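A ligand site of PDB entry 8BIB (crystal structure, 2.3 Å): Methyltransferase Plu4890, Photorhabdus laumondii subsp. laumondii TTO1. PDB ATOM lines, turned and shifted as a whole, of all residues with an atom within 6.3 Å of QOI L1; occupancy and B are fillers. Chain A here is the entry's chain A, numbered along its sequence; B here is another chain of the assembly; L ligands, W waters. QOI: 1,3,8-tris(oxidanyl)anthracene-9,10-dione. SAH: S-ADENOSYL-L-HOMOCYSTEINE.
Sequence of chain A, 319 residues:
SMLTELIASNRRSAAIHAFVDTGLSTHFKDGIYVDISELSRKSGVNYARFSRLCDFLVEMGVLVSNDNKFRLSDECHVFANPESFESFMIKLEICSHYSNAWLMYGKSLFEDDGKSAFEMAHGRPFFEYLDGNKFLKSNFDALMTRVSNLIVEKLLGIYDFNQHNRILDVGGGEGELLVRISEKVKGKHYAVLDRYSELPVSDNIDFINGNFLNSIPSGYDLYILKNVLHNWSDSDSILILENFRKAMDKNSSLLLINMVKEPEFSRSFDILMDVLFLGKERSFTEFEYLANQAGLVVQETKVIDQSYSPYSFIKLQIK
Water W2 lies within hydrogen-bond range of the backbone carbonyl oxygen of Met 89 (2.7 Å), an oxygen (O19) of QOI L1 (2.7 Å) and the side-chain carboxylate of Glu 93 (2.8 Å).
Met 89 touches QOI L1 (CG to O16, 3.8 Å).
Phe 140 touches QOI L1 (CE1 to O18, 3.4 Å).
Leu 143 touches QOI L1.
CE of Met 144 touches C7 of QOI L1, at 3.6 Å.
Val 147 touches QOI L1 (CG1 to C6, 3.8 Å).
Asn 227 touches QOI L1 (CB to O17, 3.7 Å).
SD of Met 259 touches C1 of QOI L1, 3.3 Å away.
Phe 269 touches QOI L1 (CZ to C7, 3.6 Å).
Leu 272 touches QOI L1 (CD2 to C12, 3.8 Å).
CE of Met 273 touches O18 of QOI L1 (3.5 Å).
Leu 276 touches QOI L1.
Phe 277 touches QOI L1.
Tyr 308 touches QOI L1.
Tyr 311 touches QOI L1.
The side-chain amide oxygen (OD1) of Asn 227 sits at hydrogen-bond distance from the backbone NH (N) of Met 259, 3.4 Å away.
OH of Tyr 311 is in hydrogen-bond range of OH of Tyr 308, 2.7 Å away.
SD of Met 273 sits close to OD1 of Asn 231.
OH of Tyr 311 sits at hydrogen-bond distance from ND2 of Asn 227, at 2.9 Å.
ND1 of His 230 lies within hydrogen-bond range of OD1 of Asn 231 (3.3 Å).
O17 of QOI L1 lies within hydrogen-bond range of NE2 of His 230, at 3.2 Å.
OH of Tyr 98 sits at hydrogen-bond distance from O19 of QOI L1.
The backbone carbonyl oxygen of Met 144 sits close to an oxygen (O) of SAH L2 (3.0 Å).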
ATOM      1  N   PHE A  85     -23.523 -21.861  14.806  1.00  0.00           N
ATOM      2  CA  PHE A  85     -23.012 -21.956  16.198  1.00  0.00           C
ATOM      3  C   PHE A  85     -24.118 -21.562  17.176  1.00  0.00           C
ATOM      4  O   PHE A  85     -24.112 -22.072  18.317  1.00  0.00           O
ATOM      5  CB  PHE A  85     -21.737 -21.111  16.378  1.00  0.00           C
ATOM      6  CG  PHE A  85     -21.892 -19.854  17.192  1.00  0.00           C
ATOM      7  CD1 PHE A  85     -21.736 -19.886  18.569  1.00  0.00           C
ATOM      8  CD2 PHE A  85     -22.152 -18.638  16.589  1.00  0.00           C
ATOM      9  CE1 PHE A  85     -21.871 -18.736  19.337  1.00  0.00           C
ATOM     10  CE2 PHE A  85     -22.277 -17.479  17.353  1.00  0.00           C
ATOM     11  CZ  PHE A  85     -22.133 -17.535  18.718  1.00  0.00           C
ATOM     12  N   MET A  89     -25.567 -23.575  20.417  1.00  0.00           N
ATOM     13  CA  MET A  89     -25.556 -22.808  21.686  1.00  0.00           C
ATOM     14  C   MET A  89     -26.841 -23.098  22.473  1.00  0.00           C
ATOM     15  O   MET A  89     -26.727 -23.505  23.640  1.00  0.00           O
ATOM     16  CB  MET A  89     -25.442 -21.299  21.423  1.00  0.00           C
ATOM     17  CG  MET A  89     -25.111 -20.493  22.662  1.00  0.00           C
ATOM     18  SD  MET A  89     -25.174 -18.712  22.378  1.00  0.00           S
ATOM     19  CE  MET A  89     -25.257 -18.126  24.064  1.00  0.00           C
ATOM     20  N   LEU A  92     -27.402 -26.687  23.844  1.00  0.00           N
ATOM     21  CA  LEU A  92     -26.614 -26.925  25.086  1.00  0.00           C
ATOM     22  C   LEU A  92     -27.166 -26.078  26.232  1.00  0.00           C
ATOM     23  O   LEU A  92     -27.179 -26.577  27.373  1.00  0.00           O
ATOM     24  CB  LEU A  92     -25.137 -26.592  24.826  1.00  0.00           C
ATOM     25  CG  LEU A  92     -24.331 -27.638  24.057  1.00  0.00           C
ATOM     26  CD1 LEU A  92     -22.949 -27.115  23.735  1.00  0.00           C
ATOM     27  CD2 LEU A  92     -24.231 -28.952  24.830  1.00  0.00           C
ATOM     28  N   GLU A  93     -27.599 -24.844  25.947  1.00  0.00           N
ATOM     29  CA  GLU A  93     -27.892 -23.792  26.959  1.00  0.00           C
ATOM     30  C   GLU A  93     -28.837 -24.335  28.040  1.00  0.00           C
ATOM     31  O   GLU A  93     -28.471 -24.210  29.232  1.00  0.00           O
ATOM     32  CB  GLU A  93     -28.484 -22.547  26.296  1.00  0.00           C
ATOM     33  CG  GLU A  93     -28.475 -21.324  27.199  1.00  0.00           C
ATOM     34  CD  GLU A  93     -27.090 -20.800  27.561  1.00  0.00           C
ATOM     35  OE1 GLU A  93     -26.241 -20.665  26.658  1.00  0.00           O
ATOM     36  OE2 GLU A  93     -26.860 -20.527  28.763  1.00  0.00           O
ATOM     37  N   TYR A  98     -27.100 -29.032  31.904  1.00  0.00           N
ATOM     38  CA  TYR A  98     -26.860 -27.601  32.223  1.00  0.00           C
ATOM     39  C   TYR A  98     -27.857 -27.145  33.302  1.00  0.00           C
ATOM     40  O   TYR A  98     -27.431 -26.453  34.254  1.00  0.00           O
ATOM     41  CB  TYR A  98     -26.974 -26.729  30.971  1.00  0.00           C
ATOM     42  CG  TYR A  98     -25.706 -26.621  30.168  1.00  0.00           C
ATOM     43  CD1 TYR A  98     -25.161 -25.378  29.861  1.00  0.00           C
ATOM     44  CD2 TYR A  98     -25.038 -27.745  29.708  1.00  0.00           C
ATOM     45  CE1 TYR A  98     -24.006 -25.265  29.116  1.00  0.00           C
ATOM     46  CE2 TYR A  98     -23.873 -27.642  28.964  1.00  0.00           C
ATOM     47  CZ  TYR A  98     -23.358 -26.398  28.662  1.00  0.00           C
ATOM     48  OH  TYR A  98     -22.210 -26.292  27.931  1.00  0.00           O
ATOM     49  N   PHE A 126     -16.451 -31.268  33.894  1.00  0.00           N
ATOM     50  CA  PHE A 126     -17.178 -31.106  32.601  1.00  0.00           C
ATOM     51  C   PHE A 126     -16.578 -32.008  31.517  1.00  0.00           C
ATOM     52  O   PHE A 126     -17.322 -32.848  30.966  1.00  0.00           O
ATOM     53  CB  PHE A 126     -17.165 -29.635  32.144  1.00  0.00           C
ATOM     54  CG  PHE A 126     -18.063 -29.347  30.968  1.00  0.00           C
ATOM     55  CD1 PHE A 126     -19.424 -29.116  31.159  1.00  0.00           C
ATOM     56  CD2 PHE A 126     -17.558 -29.299  29.681  1.00  0.00           C
ATOM     57  CE1 PHE A 126     -20.247 -28.850  30.083  1.00  0.00           C
ATOM     58  CE2 PHE A 126     -18.393 -29.036  28.597  1.00  0.00           C
ATOM     59  CZ  PHE A 126     -19.741 -28.809  28.808  1.00  0.00           C
ATOM     60  N   PHE A 140     -20.869 -29.604  21.955  1.00  0.00           N
ATOM     61  CA  PHE A 140     -19.820 -28.697  22.501  1.00  0.00           C
ATOM     62  C   PHE A 140     -18.698 -28.554  21.468  1.00  0.00           C
ATOM     63  O   PHE A 140     -18.366 -27.404  21.107  1.00  0.00           O
ATOM     64  CB  PHE A 140     -19.270 -29.206  23.830  1.00  0.00           C
ATOM     65  CG  PHE A 140     -18.250 -28.289  24.451  1.00  0.00           C
ATOM     66  CD1 PHE A 140     -18.651 -27.249  25.284  1.00  0.00           C
ATOM     67  CD2 PHE A 140     -16.896 -28.436  24.194  1.00  0.00           C
ATOM     68  CE1 PHE A 140     -17.712 -26.390  25.851  1.00  0.00           C
ATOM     69  CE2 PHE A 140     -15.968 -27.579  24.753  1.00  0.00           C
ATOM     70  CZ  PHE A 140     -16.381 -26.561  25.584  1.00  0.00           C
ATOM     71  N   LEU A 143     -19.825 -26.626  18.472  1.00  0.00           N
ATOM     72  CA  LEU A 143     -19.904 -25.172  18.815  1.00  0.00           C
ATOM     73  C   LEU A 143     -18.503 -24.557  18.737  1.00  0.00           C
ATOM     74  O   LEU A 143     -18.348 -23.542  18.033  1.00  0.00           O
ATOM     75  CB  LEU A 143     -20.518 -25.002  20.213  1.00  0.00           C
ATOM     76  CG  LEU A 143     -21.219 -23.674  20.481  1.00  0.00           C
ATOM     77  CD1 LEU A 143     -22.155 -23.777  21.673  1.00  0.00           C
ATOM     78  CD2 LEU A 143     -20.236 -22.535  20.684  1.00  0.00           C
ATOM     79  N   MET A 144     -17.520 -25.181  19.398  1.00  0.00           N
ATOM     80  CA  MET A 144     -16.098 -24.735  19.419  1.00  0.00           C
ATOM     81  C   MET A 144     -15.553 -24.655  17.990  1.00  0.00           C
ATOM     82  O   MET A 144     -14.760 -23.735  17.708  1.00  0.00           O
ATOM     83  CB  MET A 144     -15.212 -25.691  20.235  1.00  0.00           C
ATOM     84  CG  MET A 144     -15.491 -25.684  21.733  1.00  0.00           C
ATOM     85  SD  MET A 144     -15.670 -24.037  22.457  1.00  0.00           S
ATOM     86  CE  MET A 144     -17.452 -23.971  22.637  1.00  0.00           C
ATOM     87  N   VAL A 147     -17.204 -21.437  15.974  1.00  0.00           N
ATOM     88  CA  VAL A 147     -16.619 -20.140  16.457  1.00  0.00           C
ATOM     89  C   VAL A 147     -15.156 -20.059  16.010  1.00  0.00           C
ATOM     90  O   VAL A 147     -14.692 -18.935  15.731  1.00  0.00           O
ATOM     91  CB  VAL A 147     -16.767 -19.936  17.981  1.00  0.00           C
ATOM     92  CG1 VAL A 147     -18.230 -19.809  18.388  1.00  0.00           C
ATOM     93  CG2 VAL A 147     -16.078 -21.021  18.793  1.00  0.00           C
ATOM     94  N   ASN A 227      -9.427 -20.002  23.719  1.00  0.00           N
ATOM     95  CA  ASN A 227     -10.634 -20.288  24.555  1.00  0.00           C
ATOM     96  C   ASN A 227     -10.385 -21.528  25.430  1.00  0.00           C
ATOM     97  O   ASN A 227     -11.242 -22.442  25.415  1.00  0.00           O
ATOM     98  CB  ASN A 227     -11.883 -20.458  23.686  1.00  0.00           C
ATOM     99  CG  ASN A 227     -12.265 -19.205  22.934  1.00  0.00           C
ATOM    100  OD1 ASN A 227     -12.060 -18.091  23.416  1.00  0.00           O
ATOM    101  ND2 ASN A 227     -12.823 -19.362  21.751  1.00  0.00           N
ATOM    102  N   HIS A 230     -10.244 -19.720  30.243  1.00  0.00           N
ATOM    103  CA  HIS A 230     -11.535 -19.319  30.868  1.00  0.00           C
ATOM    104  C   HIS A 230     -12.318 -20.559  31.338  1.00  0.00           C
ATOM    105  O   HIS A 230     -13.366 -20.372  31.998  1.00  0.00           O
ATOM    106  CB  HIS A 230     -12.337 -18.384  29.939  1.00  0.00           C
ATOM    107  CG  HIS A 230     -12.857 -18.990  28.682  1.00  0.00           C
ATOM    108  ND1 HIS A 230     -12.523 -20.256  28.254  1.00  0.00           N
ATOM    109  CD2 HIS A 230     -13.666 -18.482  27.722  1.00  0.00           C
ATOM    110  CE1 HIS A 230     -13.126 -20.515  27.118  1.00  0.00           C
ATOM    111  NE2 HIS A 230     -13.828 -19.432  26.763  1.00  0.00           N
ATOM    112  N   ASN A 231     -11.819 -21.762  31.044  1.00  0.00           N
ATOM    113  CA  ASN A 231     -12.341 -23.051  31.582  1.00  0.00           C
ATOM    114  C   ASN A 231     -11.531 -23.493  32.807  1.00  0.00           C
ATOM    115  O   ASN A 231     -11.702 -24.653  33.230  1.00  0.00           O
ATOM    116  CB  ASN A 231     -12.308 -24.170  30.536  1.00  0.00           C
ATOM    117  CG  ASN A 231     -13.000 -23.813  29.233  1.00  0.00           C
ATOM    118  OD1 ASN A 231     -13.962 -23.049  29.224  1.00  0.00           O
ATOM    119  ND2 ASN A 231     -12.524 -24.374  28.141  1.00  0.00           N
ATOM    120  N   MET A 259     -11.877 -14.923  24.508  1.00  0.00           N
ATOM    121  CA  MET A 259     -12.953 -13.949  24.835  1.00  0.00           C
ATOM    122  C   MET A 259     -12.486 -13.131  26.038  1.00  0.00           C
ATOM    123  O   MET A 259     -11.992 -13.746  27.006  1.00  0.00           O
ATOM    124  CB  MET A 259     -14.267 -14.661  25.181  1.00  0.00           C
ATOM    125  CG  MET A 259     -14.921 -15.344  23.989  1.00  0.00           C
ATOM    126  SD  MET A 259     -16.275 -16.442  24.476  1.00  0.00           S
ATOM    127  CE  MET A 259     -17.416 -15.267  25.208  1.00  0.00           C
ATOM    128  N   PHE A 269     -21.808 -14.852  30.817  1.00  0.00           N
ATOM    129  CA  PHE A 269     -20.847 -15.915  30.408  1.00  0.00           C
ATOM    130  C   PHE A 269     -19.881 -16.207  31.564  1.00  0.00           C
ATOM    131  O   PHE A 269     -19.532 -17.396  31.754  1.00  0.00           O
ATOM    132  CB  PHE A 269     -20.076 -15.512  29.143  1.00  0.00           C
ATOM    133  CG  PHE A 269     -19.256 -16.621  28.549  1.00  0.00           C
ATOM    134  CD1 PHE A 269     -19.828 -17.533  27.675  1.00  0.00           C
ATOM    135  CD2 PHE A 269     -17.914 -16.772  28.886  1.00  0.00           C
ATOM    136  CE1 PHE A 269     -19.069 -18.565  27.131  1.00  0.00           C
ATOM    137  CE2 PHE A 269     -17.165 -17.795  28.340  1.00  0.00           C
ATOM    138  CZ  PHE A 269     -17.738 -18.696  27.464  1.00  0.00           C
ATOM    139  N   LEU A 272     -21.539 -18.692  33.775  1.00  0.00           N
ATOM    140  CA  LEU A 272     -21.617 -20.025  33.106  1.00  0.00           C
ATOM    141  C   LEU A 272     -20.275 -20.753  33.286  1.00  0.00           C
ATOM    142  O   LEU A 272     -20.312 -21.965  33.597  1.00  0.00           O
ATOM    143  CB  LEU A 272     -21.948 -19.861  31.622  1.00  0.00           C
ATOM    144  CG  LEU A 272     -22.180 -21.170  30.865  1.00  0.00           C
ATOM    145  CD1 LEU A 272     -23.421 -21.880  31.356  1.00  0.00           C
ATOM    146  CD2 LEU A 272     -22.269 -20.924  29.361  1.00  0.00           C
ATOM    147  N   MET A 273     -19.157 -20.053  33.122  1.00  0.00           N
ATOM    148  CA  MET A 273     -17.784 -20.613  33.270  1.00  0.00           C
ATOM    149  C   MET A 273     -17.555 -21.037  34.729  1.00  0.00           C
ATOM    150  O   MET A 273     -16.823 -22.027  34.937  1.00  0.00           O
ATOM    151  CB  MET A 273     -16.705 -19.591  32.859  1.00  0.00           C
ATOM    152  CG  MET A 273     -16.680 -19.289  31.362  1.00  0.00           C
ATOM    153  SD  MET A 273     -16.513 -20.776  30.330  1.00  0.00           S
ATOM    154  CE  MET A 273     -18.230 -21.115  29.944  1.00  0.00           C
ATOM    155  N   LEU A 276     -19.970 -24.412  35.046  1.00  0.00           N
ATOM    156  CA  LEU A 276     -19.517 -25.587  34.245  1.00  0.00           C
ATOM    157  C   LEU A 276     -18.118 -26.031  34.680  1.00  0.00           C
ATOM    158  O   LEU A 276     -17.903 -27.257  34.787  1.00  0.00           O
ATOM    159  CB  LEU A 276     -19.540 -25.243  32.754  1.00  0.00           C
ATOM    160  CG  LEU A 276     -20.907 -24.921  32.149  1.00  0.00           C
ATOM    161  CD1 LEU A 276     -20.769 -24.604  30.662  1.00  0.00           C
ATOM    162  CD2 LEU A 276     -21.900 -26.066  32.351  1.00  0.00           C
ATOM    163  N   PHE A 277     -17.198 -25.087  34.898  1.00  0.00           N
ATOM    164  CA  PHE A 277     -15.736 -25.341  34.983  1.00  0.00           C
ATOM    165  C   PHE A 277     -15.108 -24.852  36.299  1.00  0.00           C
ATOM    166  O   PHE A 277     -13.957 -25.256  36.562  1.00  0.00           O
ATOM    167  CB  PHE A 277     -15.023 -24.661  33.814  1.00  0.00           C
ATOM    168  CG  PHE A 277     -15.513 -25.097  32.460  1.00  0.00           C
ATOM    169  CD1 PHE A 277     -15.227 -26.360  31.975  1.00  0.00           C
ATOM    170  CD2 PHE A 277     -16.257 -24.238  31.660  1.00  0.00           C
ATOM    171  CE1 PHE A 277     -15.689 -26.772  30.736  1.00  0.00           C
ATOM    172  CE2 PHE A 277     -16.710 -24.641  30.417  1.00  0.00           C
ATOM    173  CZ  PHE A 277     -16.420 -25.908  29.954  1.00  0.00           C
ATOM    174  N   TYR A 308     -20.464 -11.934  18.749  1.00  0.00           N
ATOM    175  CA  TYR A 308     -20.996 -12.372  20.060  1.00  0.00           C
ATOM    176  C   TYR A 308     -20.187 -11.798  21.228  1.00  0.00           C
ATOM    177  O   TYR A 308     -20.777 -11.596  22.307  1.00  0.00           O
ATOM    178  CB  TYR A 308     -21.077 -13.901  20.145  1.00  0.00           C
ATOM    179  CG  TYR A 308     -19.783 -14.637  19.872  1.00  0.00           C
ATOM    180  CD1 TYR A 308     -18.828 -14.791  20.862  1.00  0.00           C
ATOM    181  CD2 TYR A 308     -19.532 -15.187  18.623  1.00  0.00           C
ATOM    182  CE1 TYR A 308     -17.651 -15.470  20.611  1.00  0.00           C
ATOM    183  CE2 TYR A 308     -18.356 -15.859  18.360  1.00  0.00           C
ATOM    184  CZ  TYR A 308     -17.410 -16.000  19.358  1.00  0.00           C
ATOM    185  OH  TYR A 308     -16.243 -16.670  19.106  1.00  0.00           O
ATOM    186  N   TYR A 311     -12.576 -10.302  21.503  1.00  0.00           N
ATOM    187  CA  TYR A 311     -11.474 -11.267  21.739  1.00  0.00           C
ATOM    188  C   TYR A 311     -10.186 -10.517  22.093  1.00  0.00           C
ATOM    189  O   TYR A 311     -10.033  -9.344  21.680  1.00  0.00           O
ATOM    190  CB  TYR A 311     -11.268 -12.180  20.531  1.00  0.00           C
ATOM    191  CG  TYR A 311     -12.035 -13.470  20.581  1.00  0.00           C
ATOM    192  CD1 TYR A 311     -11.400 -14.672  20.856  1.00  0.00           C
ATOM    193  CD2 TYR A 311     -13.396 -13.497  20.352  1.00  0.00           C
ATOM    194  CE1 TYR A 311     -12.093 -15.866  20.908  1.00  0.00           C
ATOM    195  CE2 TYR A 311     -14.110 -14.684  20.395  1.00  0.00           C
ATOM    196  CZ  TYR A 311     -13.464 -15.873  20.675  1.00  0.00           C
ATOM    197  OH  TYR A 311     -14.158 -17.049  20.721  1.00  0.00           O
ATOM    198  N   ARG B  11     -29.730 -17.724  31.947  1.00  0.00           N
ATOM    199  CA  ARG B  11     -28.629 -17.371  32.880  1.00  0.00           C
ATOM    200  C   ARG B  11     -29.114 -16.331  33.895  1.00  0.00           C
ATOM    201  O   ARG B  11     -28.667 -16.400  35.057  1.00  0.00           O
ATOM    202  CB  ARG B  11     -27.396 -16.879  32.106  1.00  0.00           C
ATOM    203  CG  ARG B  11     -26.764 -17.927  31.196  1.00  0.00           C
ATOM    204  CD  ARG B  11     -25.496 -17.427  30.520  1.00  0.00           C
ATOM    205  NE  ARG B  11     -25.171 -18.216  29.340  1.00  0.00           N
ATOM    206  CZ  ARG B  11     -24.235 -17.900  28.444  1.00  0.00           C
ATOM    207  NH1 ARG B  11     -24.019 -18.689  27.408  1.00  0.00           N
ATOM    208  NH2 ARG B  11     -23.515 -16.795  28.583  1.00  0.00           N
HETATM  209  C4  QOI L   1     -19.074 -20.165  23.448  1.00  0.00           C
HETATM  210  C5  QOI L   1     -19.044 -19.241  22.401  1.00  0.00           C
HETATM  211  C6  QOI L   1     -17.839 -18.700  21.975  1.00  0.00           C
HETATM  212  C7  QOI L   1     -17.886 -21.469  25.121  1.00  0.00           C
HETATM  213  C8  QOI L   1     -19.103 -22.013  25.539  1.00  0.00           C
HETATM  214  C10 QOI L   1     -20.281 -20.709  23.865  1.00  0.00           C
HETATM  215  C13 QOI L   1     -20.369 -23.479  27.007  1.00  0.00           C
HETATM  216  O16 QOI L   1     -21.335 -20.364  23.319  1.00  0.00           O
HETATM  217  C9  QOI L   1     -20.299 -21.630  24.920  1.00  0.00           C
HETATM  218  C11 QOI L   1     -21.514 -22.170  25.347  1.00  0.00           C
HETATM  219  C12 QOI L   1     -21.545 -23.096  26.385  1.00  0.00           C
HETATM  220  O19 QOI L   1     -22.734 -23.615  26.781  1.00  0.00           O
HETATM  221  C14 QOI L   1     -19.164 -22.938  26.581  1.00  0.00           C
HETATM  222  O18 QOI L   1     -17.982 -23.288  27.171  1.00  0.00           O
HETATM  223  O15 QOI L   1     -16.832 -21.804  25.664  1.00  0.00           O
HETATM  224  C3  QOI L   1     -17.868 -20.548  24.066  1.00  0.00           C
HETATM  225  C1  QOI L   1     -16.645 -19.077  22.581  1.00  0.00           C
HETATM  226  C2  QOI L   1     -16.665 -19.991  23.625  1.00  0.00           C
HETATM  227  O17 QOI L   1     -15.520 -20.375  24.241  1.00  0.00           O
HETATM  228  N   SAH L   2      -9.367 -24.295  21.296  1.00  0.00           N
HETATM  229  CA  SAH L   2     -10.706 -24.748  20.821  1.00  0.00           C
HETATM  230  CB  SAH L   2     -11.488 -25.456  21.935  1.00  0.00           C
HETATM  231  CG  SAH L   2     -11.669 -24.640  23.200  1.00  0.00           C
HETATM  232  SD  SAH L   2     -12.689 -25.471  24.441  1.00  0.00           S
HETATM  233  C   SAH L   2     -11.514 -23.528  20.336  1.00  0.00           C
HETATM  234  O   SAH L   2     -12.514 -23.664  19.639  1.00  0.00           O
HETATM  235  OXT SAH L   2     -11.173 -22.390  20.642  1.00  0.00           O
HETATM  236  C5' SAH L   2     -11.438 -26.179  25.548  1.00  0.00           C
HETATM  237  C4' SAH L   2     -10.732 -27.383  24.957  1.00  0.00           C
HETATM  238  O4' SAH L   2      -9.697 -27.830  25.863  1.00  0.00           O
HETATM  239  C3' SAH L   2     -11.634 -28.588  24.698  1.00  0.00           C
HETATM  240  O3' SAH L   2     -11.496 -29.032  23.351  1.00  0.00           O
HETATM  241  C2' SAH L   2     -11.140 -29.644  25.690  1.00  0.00           C
HETATM  242  O2' SAH L   2     -11.260 -30.957  25.201  1.00  0.00           O
HETATM  243  C1' SAH L   2      -9.677 -29.230  25.852  1.00  0.00           C
HETATM  244  N9  SAH L   2      -9.067 -29.700  27.096  1.00  0.00           N
HETATM  245  C8  SAH L   2      -9.615 -29.644  28.348  1.00  0.00           C
HETATM  246  N7  SAH L   2      -8.829 -30.129  29.284  1.00  0.00           N
HETATM  247  C5  SAH L   2      -7.700 -30.529  28.600  1.00  0.00           C
HETATM  248  C6  SAH L   2      -6.497 -31.112  29.034  1.00  0.00           C
HETATM  249  N6  SAH L   2      -6.232 -31.413  30.304  1.00  0.00           N
HETATM  250  N1  SAH L   2      -5.553 -31.381  28.098  1.00  0.00           N
HETATM  251  C2  SAH L   2      -5.819 -31.073  26.815  1.00  0.00           C
HETATM  252  N3  SAH L   2      -6.914 -30.514  26.297  1.00  0.00           N
HETATM  253  C4  SAH L   2      -7.826 -30.262  27.243  1.00  0.00           C
HETATM  254  O   HOH W   1     -14.417 -23.302  25.858  1.00  0.00           O
HETATM  255  O   HOH W   2     -24.949 -22.847  25.504  1.00  0.00           O
